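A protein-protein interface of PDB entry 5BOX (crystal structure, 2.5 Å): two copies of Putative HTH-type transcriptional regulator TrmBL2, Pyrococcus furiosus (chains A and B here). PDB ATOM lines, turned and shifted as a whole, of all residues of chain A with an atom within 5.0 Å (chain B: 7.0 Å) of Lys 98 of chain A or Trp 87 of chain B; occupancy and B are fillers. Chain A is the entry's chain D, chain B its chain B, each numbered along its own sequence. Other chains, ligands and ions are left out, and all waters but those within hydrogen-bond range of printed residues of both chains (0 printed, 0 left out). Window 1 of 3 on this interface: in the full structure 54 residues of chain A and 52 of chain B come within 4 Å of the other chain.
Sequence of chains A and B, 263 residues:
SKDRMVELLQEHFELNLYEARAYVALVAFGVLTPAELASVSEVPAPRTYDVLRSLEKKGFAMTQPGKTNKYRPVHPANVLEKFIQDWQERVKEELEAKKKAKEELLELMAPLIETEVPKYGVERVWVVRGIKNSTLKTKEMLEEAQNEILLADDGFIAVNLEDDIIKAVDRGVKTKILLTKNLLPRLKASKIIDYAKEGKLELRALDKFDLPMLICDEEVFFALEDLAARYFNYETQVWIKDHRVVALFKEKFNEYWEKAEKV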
ATOM      1  N   VAL A  91     -19.162  -7.011  14.654  1.00  0.00           N
ATOM      2  CA  VAL A  91     -18.687  -8.190  15.367  1.00  0.00           C
ATOM      3  C   VAL A  91     -19.754  -9.268  15.335  1.00  0.00           C
ATOM      4  O   VAL A  91     -19.456 -10.438  15.110  1.00  0.00           O
ATOM      5  CB  VAL A  91     -18.303  -7.859  16.826  1.00  0.00           C
ATOM      6  CG1 VAL A  91     -17.246  -6.764  16.867  1.00  0.00           C
ATOM      7  CG2 VAL A  91     -19.535  -7.458  17.631  1.00  0.00           C
ATOM      8  N   GLU A  94     -19.646 -10.940  12.121  1.00  0.00           N
ATOM      9  CA  GLU A  94     -18.473 -11.790  12.021  1.00  0.00           C
ATOM     10  C   GLU A  94     -18.726 -13.079  12.794  1.00  0.00           C
ATOM     11  O   GLU A  94     -18.238 -14.145  12.419  1.00  0.00           O
ATOM     12  CB  GLU A  94     -17.234 -11.070  12.555  1.00  0.00           C
ATOM     13  CG  GLU A  94     -15.929 -11.783  12.262  1.00  0.00           C
ATOM     14  CD  GLU A  94     -14.739 -11.032  12.812  1.00  0.00           C
ATOM     15  OE1 GLU A  94     -14.932  -9.884  13.264  1.00  0.00           O
ATOM     16  OE2 GLU A  94     -13.616 -11.582  12.794  1.00  0.00           O
ATOM     17  N   LEU A  95     -19.499 -12.973  13.871  1.00  0.00           N
ATOM     18  CA  LEU A  95     -19.872 -14.140  14.656  1.00  0.00           C
ATOM     19  C   LEU A  95     -20.660 -15.113  13.796  1.00  0.00           C
ATOM     20  O   LEU A  95     -20.355 -16.305  13.757  1.00  0.00           O
ATOM     21  CB  LEU A  95     -20.684 -13.733  15.884  1.00  0.00           C
ATOM     22  CG  LEU A  95     -21.239 -14.887  16.720  1.00  0.00           C
ATOM     23  CD1 LEU A  95     -20.106 -15.794  17.175  1.00  0.00           C
ATOM     24  CD2 LEU A  95     -22.018 -14.365  17.918  1.00  0.00           C
ATOM     25  N   GLU A  96     -21.659 -14.590  13.091  1.00  0.00           N
ATOM     26  CA  GLU A  96     -22.475 -15.403  12.192  1.00  0.00           C
ATOM     27  C   GLU A  96     -21.592 -16.064  11.141  1.00  0.00           C
ATOM     28  O   GLU A  96     -21.727 -17.253  10.861  1.00  0.00           O
ATOM     29  CB  GLU A  96     -23.562 -14.558  11.521  1.00  0.00           C
ATOM     30  CG  GLU A  96     -24.564 -13.926  12.479  1.00  0.00           C
ATOM     31  CD  GLU A  96     -25.502 -12.943  11.783  1.00  0.00           C
ATOM     32  OE1 GLU A  96     -25.337 -12.713  10.566  1.00  0.00           O
ATOM     33  OE2 GLU A  96     -26.400 -12.391  12.453  1.00  0.00           O
ATOM     34  N   ALA A  97     -20.682 -15.285  10.566  1.00  0.00           N
ATOM     35  CA  ALA A  97     -19.769 -15.797   9.550  1.00  0.00           C
ATOM     36  C   ALA A  97     -18.922 -16.937  10.103  1.00  0.00           C
ATOM     37  O   ALA A  97     -18.734 -17.959   9.440  1.00  0.00           O
ATOM     38  CB  ALA A  97     -18.874 -14.678   9.029  1.00  0.00           C
ATOM     39  N   LYS A  98     -18.421 -16.750  11.321  1.00  0.00           N
ATOM     40  CA  LYS A  98     -17.595 -17.745  11.997  1.00  0.00           C
ATOM     41  C   LYS A  98     -18.370 -19.034  12.221  1.00  0.00           C
ATOM     42  O   LYS A  98     -17.872 -20.128  11.948  1.00  0.00           O
ATOM     43  CB  LYS A  98     -17.086 -17.202  13.334  1.00  0.00           C
ATOM     44  CG  LYS A  98     -15.733 -16.522  13.250  1.00  0.00           C
ATOM     45  CD  LYS A  98     -15.344 -15.877  14.575  1.00  0.00           C
ATOM     46  CE  LYS A  98     -13.937 -15.312  14.504  1.00  0.00           C
ATOM     47  NZ  LYS A  98     -13.734 -14.588  13.216  1.00  0.00           N
ATOM     48  N   LYS A  99     -19.590 -18.894  12.725  1.00  0.00           N
ATOM     49  CA  LYS A  99     -20.451 -20.040  12.958  1.00  0.00           C
ATOM     50  C   LYS A  99     -20.723 -20.769  11.650  1.00  0.00           C
ATOM     51  O   LYS A  99     -20.775 -21.999  11.618  1.00  0.00           O
ATOM     52  CB  LYS A  99     -21.768 -19.609  13.604  1.00  0.00           C
ATOM     53  CG  LYS A  99     -21.632 -19.053  15.011  1.00  0.00           C
ATOM     54  CD  LYS A  99     -23.001 -18.827  15.638  1.00  0.00           C
ATOM     55  CE  LYS A  99     -22.889 -18.354  17.077  1.00  0.00           C
ATOM     56  NZ  LYS A  99     -24.229 -18.189  17.708  1.00  0.00           N
ATOM     57  N   LYS A 100     -20.891 -20.013  10.569  1.00  0.00           N
ATOM     58  CA  LYS A 100     -21.155 -20.618   9.270  1.00  0.00           C
ATOM     59  C   LYS A 100     -19.920 -21.354   8.779  1.00  0.00           C
ATOM     60  O   LYS A 100     -20.025 -22.403   8.142  1.00  0.00           O
ATOM     61  CB  LYS A 100     -21.581 -19.569   8.240  1.00  0.00           C
ATOM     62  CG  LYS A 100     -22.797 -18.762   8.641  1.00  0.00           C
ATOM     63  CD  LYS A 100     -24.095 -19.482   8.304  1.00  0.00           C
ATOM     64  CE  LYS A 100     -25.295 -18.622   8.680  1.00  0.00           C
ATOM     65  NZ  LYS A 100     -26.599 -19.269   8.360  1.00  0.00           N
ATOM     66  N   ALA A 101     -18.749 -20.805   9.085  1.00  0.00           N
ATOM     67  CA  ALA A 101     -17.495 -21.429   8.682  1.00  0.00           C
ATOM     68  C   ALA A 101     -17.261 -22.713   9.463  1.00  0.00           C
ATOM     69  O   ALA A 101     -16.768 -23.699   8.917  1.00  0.00           O
ATOM     70  CB  ALA A 101     -16.340 -20.473   8.883  1.00  0.00           C
ATOM     71  N   LYS A 102     -17.649 -22.707  10.735  1.00  0.00           N
ATOM     72  CA  LYS A 102     -17.481 -23.877  11.589  1.00  0.00           C
ATOM     73  C   LYS A 102     -18.352 -25.024  11.098  1.00  0.00           C
ATOM     74  O   LYS A 102     -17.869 -26.132  10.860  1.00  0.00           O
ATOM     75  CB  LYS A 102     -17.813 -23.528  13.046  1.00  0.00           C
ATOM     76  CG  LYS A 102     -18.032 -24.726  13.971  1.00  0.00           C
ATOM     77  CD  LYS A 102     -18.306 -24.260  15.403  1.00  0.00           C
ATOM     78  CE  LYS A 102     -19.237 -25.200  16.146  1.00  0.00           C
ATOM     79  NZ  LYS A 102     -20.568 -25.292  15.478  1.00  0.00           N
ATOM     80  N   GLU B  11      -9.359 -17.961   7.607  1.00  0.00           N
ATOM     81  CA  GLU B  11     -10.224 -16.789   7.542  1.00  0.00           C
ATOM     82  C   GLU B  11     -10.973 -16.512   8.833  1.00  0.00           C
ATOM     83  O   GLU B  11     -11.336 -15.368   9.104  1.00  0.00           O
ATOM     84  CB  GLU B  11     -11.228 -16.928   6.403  1.00  0.00           C
ATOM     85  CG  GLU B  11     -12.114 -15.707   6.227  1.00  0.00           C
ATOM     86  CD  GLU B  11     -11.315 -14.440   5.977  1.00  0.00           C
ATOM     87  OE1 GLU B  11     -10.153 -14.545   5.530  1.00  0.00           O
ATOM     88  OE2 GLU B  11     -11.848 -13.339   6.237  1.00  0.00           O
ATOM     89  N   HIS B  12     -11.228 -17.550   9.624  1.00  0.00           N
ATOM     90  CA  HIS B  12     -12.107 -17.378  10.778  1.00  0.00           C
ATOM     91  C   HIS B  12     -11.555 -17.895  12.093  1.00  0.00           C
ATOM     92  O   HIS B  12     -12.138 -17.643  13.146  1.00  0.00           O
ATOM     93  CB  HIS B  12     -13.457 -18.042  10.502  1.00  0.00           C
ATOM     94  CG  HIS B  12     -14.192 -17.431   9.353  1.00  0.00           C
ATOM     95  ND1 HIS B  12     -14.820 -16.209   9.443  1.00  0.00           N
ATOM     96  CD2 HIS B  12     -14.381 -17.860   8.083  1.00  0.00           C
ATOM     97  CE1 HIS B  12     -15.373 -15.914   8.281  1.00  0.00           C
ATOM     98  NE2 HIS B  12     -15.120 -16.899   7.437  1.00  0.00           N
ATOM     99  N   PHE B  13     -10.435 -18.606  12.049  1.00  0.00           N
ATOM    100  CA  PHE B  13      -9.935 -19.227  13.264  1.00  0.00           C
ATOM    101  C   PHE B  13      -8.453 -18.973  13.517  1.00  0.00           C
ATOM    102  O   PHE B  13      -7.806 -19.719  14.250  1.00  0.00           O
ATOM    103  CB  PHE B  13     -10.240 -20.717  13.215  1.00  0.00           C
ATOM    104  CG  PHE B  13     -11.701 -21.012  13.024  1.00  0.00           C
ATOM    105  CD1 PHE B  13     -12.565 -21.043  14.114  1.00  0.00           C
ATOM    106  CD2 PHE B  13     -12.224 -21.213  11.749  1.00  0.00           C
ATOM    107  CE1 PHE B  13     -13.927 -21.306  13.940  1.00  0.00           C
ATOM    108  CE2 PHE B  13     -13.575 -21.471  11.566  1.00  0.00           C
ATOM    109  CZ  PHE B  13     -14.428 -21.519  12.666  1.00  0.00           C
ATOM    110  N   GLU B  14      -7.929 -17.914  12.908  1.00  0.00           N
ATOM    111  CA  GLU B  14      -6.607 -17.391  13.253  1.00  0.00           C
ATOM    112  C   GLU B  14      -5.498 -18.439  13.155  1.00  0.00           C
ATOM    113  O   GLU B  14      -4.643 -18.534  14.037  1.00  0.00           O
ATOM    114  CB  GLU B  14      -6.634 -16.800  14.668  1.00  0.00           C
ATOM    115  CG  GLU B  14      -7.509 -15.563  14.828  1.00  0.00           C
ATOM    116  CD  GLU B  14      -7.581 -15.082  16.270  1.00  0.00           C
ATOM    117  OE1 GLU B  14      -6.922 -15.695  17.138  1.00  0.00           O
ATOM    118  OE2 GLU B  14      -8.292 -14.088  16.540  1.00  0.00           O
ATOM    119  N   LEU B  80     -13.088 -25.632  17.365  1.00  0.00           N
ATOM    120  CA  LEU B  80     -13.699 -24.528  16.623  1.00  0.00           C
ATOM    121  C   LEU B  80     -14.757 -23.818  17.459  1.00  0.00           C
ATOM    122  O   LEU B  80     -14.840 -22.592  17.458  1.00  0.00           O
ATOM    123  CB  LEU B  80     -14.324 -25.024  15.314  1.00  0.00           C
ATOM    124  CG  LEU B  80     -13.363 -25.575  14.254  1.00  0.00           C
ATOM    125  CD1 LEU B  80     -14.107 -25.931  12.976  1.00  0.00           C
ATOM    126  CD2 LEU B  80     -12.232 -24.597  13.962  1.00  0.00           C
ATOM    127  N   GLU B  81     -15.568 -24.585  18.175  1.00  0.00           N
ATOM    128  CA  GLU B  81     -16.584 -23.975  19.019  1.00  0.00           C
ATOM    129  C   GLU B  81     -15.923 -23.293  20.203  1.00  0.00           C
ATOM    130  O   GLU B  81     -16.359 -22.226  20.628  1.00  0.00           O
ATOM    131  CB  GLU B  81     -17.608 -24.996  19.502  1.00  0.00           C
ATOM    132  CG  GLU B  81     -18.715 -24.362  20.313  1.00  0.00           C
ATOM    133  CD  GLU B  81     -19.810 -25.341  20.649  1.00  0.00           C
ATOM    134  OE1 GLU B  81     -19.790 -26.463  20.098  1.00  0.00           O
ATOM    135  OE2 GLU B  81     -20.688 -24.990  21.465  1.00  0.00           O
ATOM    136  N   LYS B  82     -14.888 -23.929  20.748  1.00  0.00           N
ATOM    137  CA  LYS B  82     -14.099 -23.350  21.838  1.00  0.00           C
ATOM    138  C   LYS B  82     -13.545 -21.990  21.410  1.00  0.00           C
ATOM    139  O   LYS B  82     -13.647 -21.004  22.143  1.00  0.00           O
ATOM    140  CB  LYS B  82     -12.959 -24.293  22.239  1.00  0.00           C
ATOM    141  CG  LYS B  82     -11.972 -23.729  23.259  1.00  0.00           C
ATOM    142  CD  LYS B  82     -12.522 -23.786  24.681  1.00  0.00           C
ATOM    143  CE  LYS B  82     -11.513 -23.231  25.682  1.00  0.00           C
ATOM    144  NZ  LYS B  82     -12.099 -23.032  27.040  1.00  0.00           N
ATOM    145  N   PHE B  83     -12.970 -21.949  20.212  1.00  0.00           N
ATOM    146  CA  PHE B  83     -12.432 -20.716  19.656  1.00  0.00           C
ATOM    147  C   PHE B  83     -13.486 -19.620  19.644  1.00  0.00           C
ATOM    148  O   PHE B  83     -13.253 -18.514  20.129  1.00  0.00           O
ATOM    149  CB  PHE B  83     -11.916 -20.954  18.238  1.00  0.00           C
ATOM    150  CG  PHE B  83     -11.430 -19.713  17.552  1.00  0.00           C
ATOM    151  CD1 PHE B  83     -12.297 -18.936  16.804  1.00  0.00           C
ATOM    152  CD2 PHE B  83     -10.104 -19.322  17.653  1.00  0.00           C
ATOM    153  CE1 PHE B  83     -11.851 -17.794  16.168  1.00  0.00           C
ATOM    154  CE2 PHE B  83      -9.651 -18.181  17.018  1.00  0.00           C
ATOM    155  CZ  PHE B  83     -10.524 -17.417  16.276  1.00  0.00           C
ATOM    156  N   ILE B  84     -14.647 -19.947  19.090  1.00  0.00           N
ATOM    157  CA  ILE B  84     -15.742 -18.999  18.952  1.00  0.00           C
ATOM    158  C   ILE B  84     -16.186 -18.479  20.314  1.00  0.00           C
ATOM    159  O   ILE B  84     -16.369 -17.277  20.498  1.00  0.00           O
ATOM    160  CB  ILE B  84     -16.911 -19.628  18.183  1.00  0.00           C
ATOM    161  CG1 ILE B  84     -16.496 -19.880  16.728  1.00  0.00           C
ATOM    162  CG2 ILE B  84     -18.145 -18.748  18.277  1.00  0.00           C
ATOM    163  CD1 ILE B  84     -17.574 -20.482  15.861  1.00  0.00           C
ATOM    164  N   GLN B  85     -16.363 -19.384  21.269  1.00  0.00           N
ATOM    165  CA  GLN B  85     -16.799 -18.993  22.601  1.00  0.00           C
ATOM    166  C   GLN B  85     -15.775 -18.077  23.271  1.00  0.00           C
ATOM    167  O   GLN B  85     -16.139 -17.075  23.891  1.00  0.00           O
ATOM    168  CB  GLN B  85     -17.043 -20.236  23.452  1.00  0.00           C
ATOM    169  CG  GLN B  85     -18.212 -21.068  22.960  1.00  0.00           C
ATOM    170  CD  GLN B  85     -18.331 -22.394  23.678  1.00  0.00           C
ATOM    171  OE1 GLN B  85     -17.452 -22.777  24.450  1.00  0.00           O
ATOM    172  NE2 GLN B  85     -19.417 -23.113  23.416  1.00  0.00           N
ATOM    173  N   ASP B  86     -14.495 -18.416  23.130  1.00  0.00           N
ATOM    174  CA  ASP B  86     -13.421 -17.571  23.649  1.00  0.00           C
ATOM    175  C   ASP B  86     -13.416 -16.206  22.974  1.00  0.00           C
ATOM    176  O   ASP B  86     -13.333 -15.173  23.639  1.00  0.00           O
ATOM    177  CB  ASP B  86     -12.059 -18.248  23.476  1.00  0.00           C
ATOM    178  CG  ASP B  86     -11.820 -19.343  24.499  1.00  0.00           C
ATOM    179  OD1 ASP B  86     -12.555 -19.379  25.512  1.00  0.00           O
ATOM    180  OD2 ASP B  86     -10.889 -20.155  24.301  1.00  0.00           O
ATOM    181  N   TRP B  87     -13.490 -16.215  21.646  1.00  0.00           N
ATOM    182  CA  TRP B  87     -13.553 -14.990  20.852  1.00  0.00           C
ATOM    183  C   TRP B  87     -14.659 -14.067  21.356  1.00  0.00           C
ATOM    184  O   TRP B  87     -14.433 -12.883  21.594  1.00  0.00           O
ATOM    185  CB  TRP B  87     -13.778 -15.341  19.384  1.00  0.00           C
ATOM    186  CG  TRP B  87     -13.890 -14.178  18.474  1.00  0.00           C
ATOM    187  CD1 TRP B  87     -12.869 -13.496  17.887  1.00  0.00           C
ATOM    188  CD2 TRP B  87     -15.101 -13.564  18.014  1.00  0.00           C
ATOM    189  NE1 TRP B  87     -13.365 -12.485  17.098  1.00  0.00           N
ATOM    190  CE2 TRP B  87     -14.734 -12.505  17.160  1.00  0.00           C
ATOM    191  CE3 TRP B  87     -16.459 -13.802  18.248  1.00  0.00           C
ATOM    192  CZ2 TRP B  87     -15.674 -11.690  16.537  1.00  0.00           C
ATOM    193  CZ3 TRP B  87     -17.390 -12.989  17.629  1.00  0.00           C
ATOM    194  CH2 TRP B  87     -16.994 -11.946  16.784  1.00  0.00           C
ATOM    195  N   GLN B  88     -15.847 -14.627  21.552  1.00  0.00           N
ATOM    196  CA  GLN B  88     -16.981 -13.864  22.058  1.00  0.00           C
ATOM    197  C   GLN B  88     -16.648 -13.224  23.397  1.00  0.00           C
ATOM    198  O   GLN B  88     -17.182 -12.175  23.748  1.00  0.00           O
ATOM    199  CB  GLN B  88     -18.220 -14.750  22.201  1.00  0.00           C
ATOM    200  CG  GLN B  88     -18.728 -15.347  20.906  1.00  0.00           C
ATOM    201  CD  GLN B  88     -20.034 -16.093  21.102  1.00  0.00           C
ATOM    202  OE1 GLN B  88     -20.052 -17.314  21.280  1.00  0.00           O
ATOM    203  NE2 GLN B  88     -21.139 -15.356  21.085  1.00  0.00           N
ATOM    204  N   GLU B  89     -15.787 -13.885  24.160  1.00  0.00           N
ATOM    205  CA  GLU B  89     -15.398 -13.376  25.465  1.00  0.00           C
ATOM    206  C   GLU B  89     -14.416 -12.211  25.313  1.00  0.00           C
ATOM    207  O   GLU B  89     -14.414 -11.277  26.119  1.00  0.00           O
ATOM    208  CB  GLU B  89     -14.776 -14.491  26.309  1.00  0.00           C
ATOM    209  CG  GLU B  89     -15.756 -15.565  26.751  1.00  0.00           C
ATOM    210  CD  GLU B  89     -16.894 -15.009  27.582  1.00  0.00           C
ATOM    211  OE1 GLU B  89     -16.777 -13.866  28.074  1.00  0.00           O
ATOM    212  OE2 GLU B  89     -17.906 -15.720  27.750  1.00  0.00           O
ATOM    213  N   ARG B  90     -13.599 -12.262  24.264  1.00  0.00           N
ATOM    214  CA  ARG B  90     -12.689 -11.167  23.957  1.00  0.00           C
ATOM    215  C   ARG B  90     -13.497  -9.964  23.513  1.00  0.00           C
ATOM    216  O   ARG B  90     -13.304  -8.850  24.005  1.00  0.00           O
ATOM    217  CB  ARG B  90     -11.689 -11.574  22.869  1.00  0.00           C
ATOM    218  CG  ARG B  90     -10.593 -12.529  23.345  1.00  0.00           C
ATOM    219  CD  ARG B  90      -9.519 -12.783  22.285  1.00  0.00           C
ATOM    220  NE  ARG B  90      -9.933 -13.742  21.262  1.00  0.00           N
ATOM    221  CZ  ARG B  90     -10.004 -15.055  21.462  1.00  0.00           C
ATOM    222  NH1 ARG B  90      -9.701 -15.560  22.650  1.00  0.00           N
ATOM    223  NH2 ARG B  90     -10.386 -15.865  20.481  1.00  0.00           N
ATOM    224  N   VAL B  91     -14.430 -10.214  22.597  1.00  0.00           N
ATOM    225  CA  VAL B  91     -15.353  -9.194  22.126  1.00  0.00           C
ATOM    226  C   VAL B  91     -16.059  -8.556  23.306  1.00  0.00           C
ATOM    227  O   VAL B  91     -16.122  -7.332  23.417  1.00  0.00           O
ATOM    228  CB  VAL B  91     -16.380  -9.787  21.146  1.00  0.00           C
ATOM    229  CG1 VAL B  91     -17.552  -8.841  20.969  1.00  0.00           C
ATOM    230  CG2 VAL B  91     -15.724 -10.098  19.811  1.00  0.00           C
ATOM    231  N   LYS B  92     -16.570  -9.390  24.204  1.00  0.00           N
ATOM    232  CA  LYS B  92     -17.288  -8.888  25.366  1.00  0.00           C
ATOM    233  C   LYS B  92     -16.397  -7.977  26.205  1.00  0.00           C
ATOM    234  O   LYS B  92     -16.892  -7.082  26.888  1.00  0.00           O
ATOM    235  CB  LYS B  92     -17.830 -10.039  26.214  1.00  0.00           C
ATOM    236  CG  LYS B  92     -18.707  -9.580  27.374  1.00  0.00           C
ATOM    237  CD  LYS B  92     -19.282 -10.759  28.145  1.00  0.00           C
ATOM    238  CE  LYS B  92     -20.125 -10.300  29.329  1.00  0.00           C
ATOM    239  NZ  LYS B  92     -20.737 -11.453  30.052  1.00  0.00           N
ATOM    240  N   GLU B  93     -15.088  -8.196  26.154  1.00  0.00           N
ATOM    241  CA  GLU B  93     -14.157  -7.347  26.894  1.00  0.00           C
ATOM    242  C   GLU B  93     -13.820  -6.076  26.120  1.00  0.00           C
ATOM    243  O   GLU B  93     -13.889  -4.971  26.659  1.00  0.00           O
ATOM    244  CB  GLU B  93     -12.872  -8.100  27.224  1.00  0.00           C
ATOM    245  CG  GLU B  93     -13.026  -9.134  28.314  1.00  0.00           C
ATOM    246  CD  GLU B  93     -11.689  -9.646  28.792  1.00  0.00           C
ATOM    247  OE1 GLU B  93     -10.656  -9.132  28.310  1.00  0.00           O
ATOM    248  OE2 GLU B  93     -11.669 -10.551  29.653  1.00  0.00           O
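NE2 of Gln 85 of chain B sits at hydrogen-bond distance from OE2 of Glu 81 of chain B. NZ of Lys 98 of chain A lies within salt-bridge range of OE2 of Glu 94 of chain A.
Position printed for both chains: 91. Of the 17 pairs that touch across the chains among the printed residues, none has its exchanged pair printed and touching as well.
The side-chain amino group of Lys 98 of chain A sits close to the backbone carbonyl oxygen of His 12 of chain B, 3.4 Å away.
Among the printed residues, merely in contact across the chains: Val 91 of chain A with Trp 87 of chain B (3.3 Å), Ala 101 of chain A with His 12 of chain B (3.4 Å), Leu 95 of chain A with Gln 88 of chain B (3.4 Å), Lys 98 of chain A with Phe 83 of chain B (3.6 Å), Leu 95 of chain A with Ile 84 of chain B (3.7 Å), Lys 102 of chain A with Glu 81 of chain B (3.7 Å), Lys 98 of chain A with Phe 13 of chain B (3.8 Å), Ala 97 of chain A with His 12 of chain B (3.8 Å), Leu 95 of chain A with Trp 87 of chain B (3.8 Å), Glu 94 of chain A with Trp 87 of chain B (3.8 Å), Lys 102 of chain A with Ile 84 of chain B (3.9 Å), Lys 98 of chain A with Trp 87 of chain B (3.9 Å), Lys 102 of chain A with Phe 13 of chain B (3.9 Å), Lys 98 of chain A with Ile 84 of chain B (3.9 Å), Lys 102 of chain A with Leu 80 of chain B (3.95 Å) and Ala 101 of chain A with Phe 13 of chain B (3.98 Å).
Of the printed residues of chain B, Lys 98 of chain A touches His 12, Phe 13, Phe 83, Ile 84 and Trp 87. Trp 87 of chain B touches four residues of chain A. Printed residues of chain A within 4 Å of His 12 of chain B: Ala 97, Lys 98 and Ala 101. Printed residues of chain A within 4 Å of Leu 80 of chain B: Lys 102. Printed residues of chain A within 4 Å of Glu 81 of chain B: Lys 102.
Printed residues of chain A that touch a printed residue of chain B: Val 91, Glu 94, Leu 95, Ala 97, Lys 98, Ala 101 and Lys 102. Hydrophobic or aromatic side chains of chain B within 4 Å of the printed part of chain A: His 12, Phe 13, Leu 80, Phe 83, Ile 84 and Trp 87.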
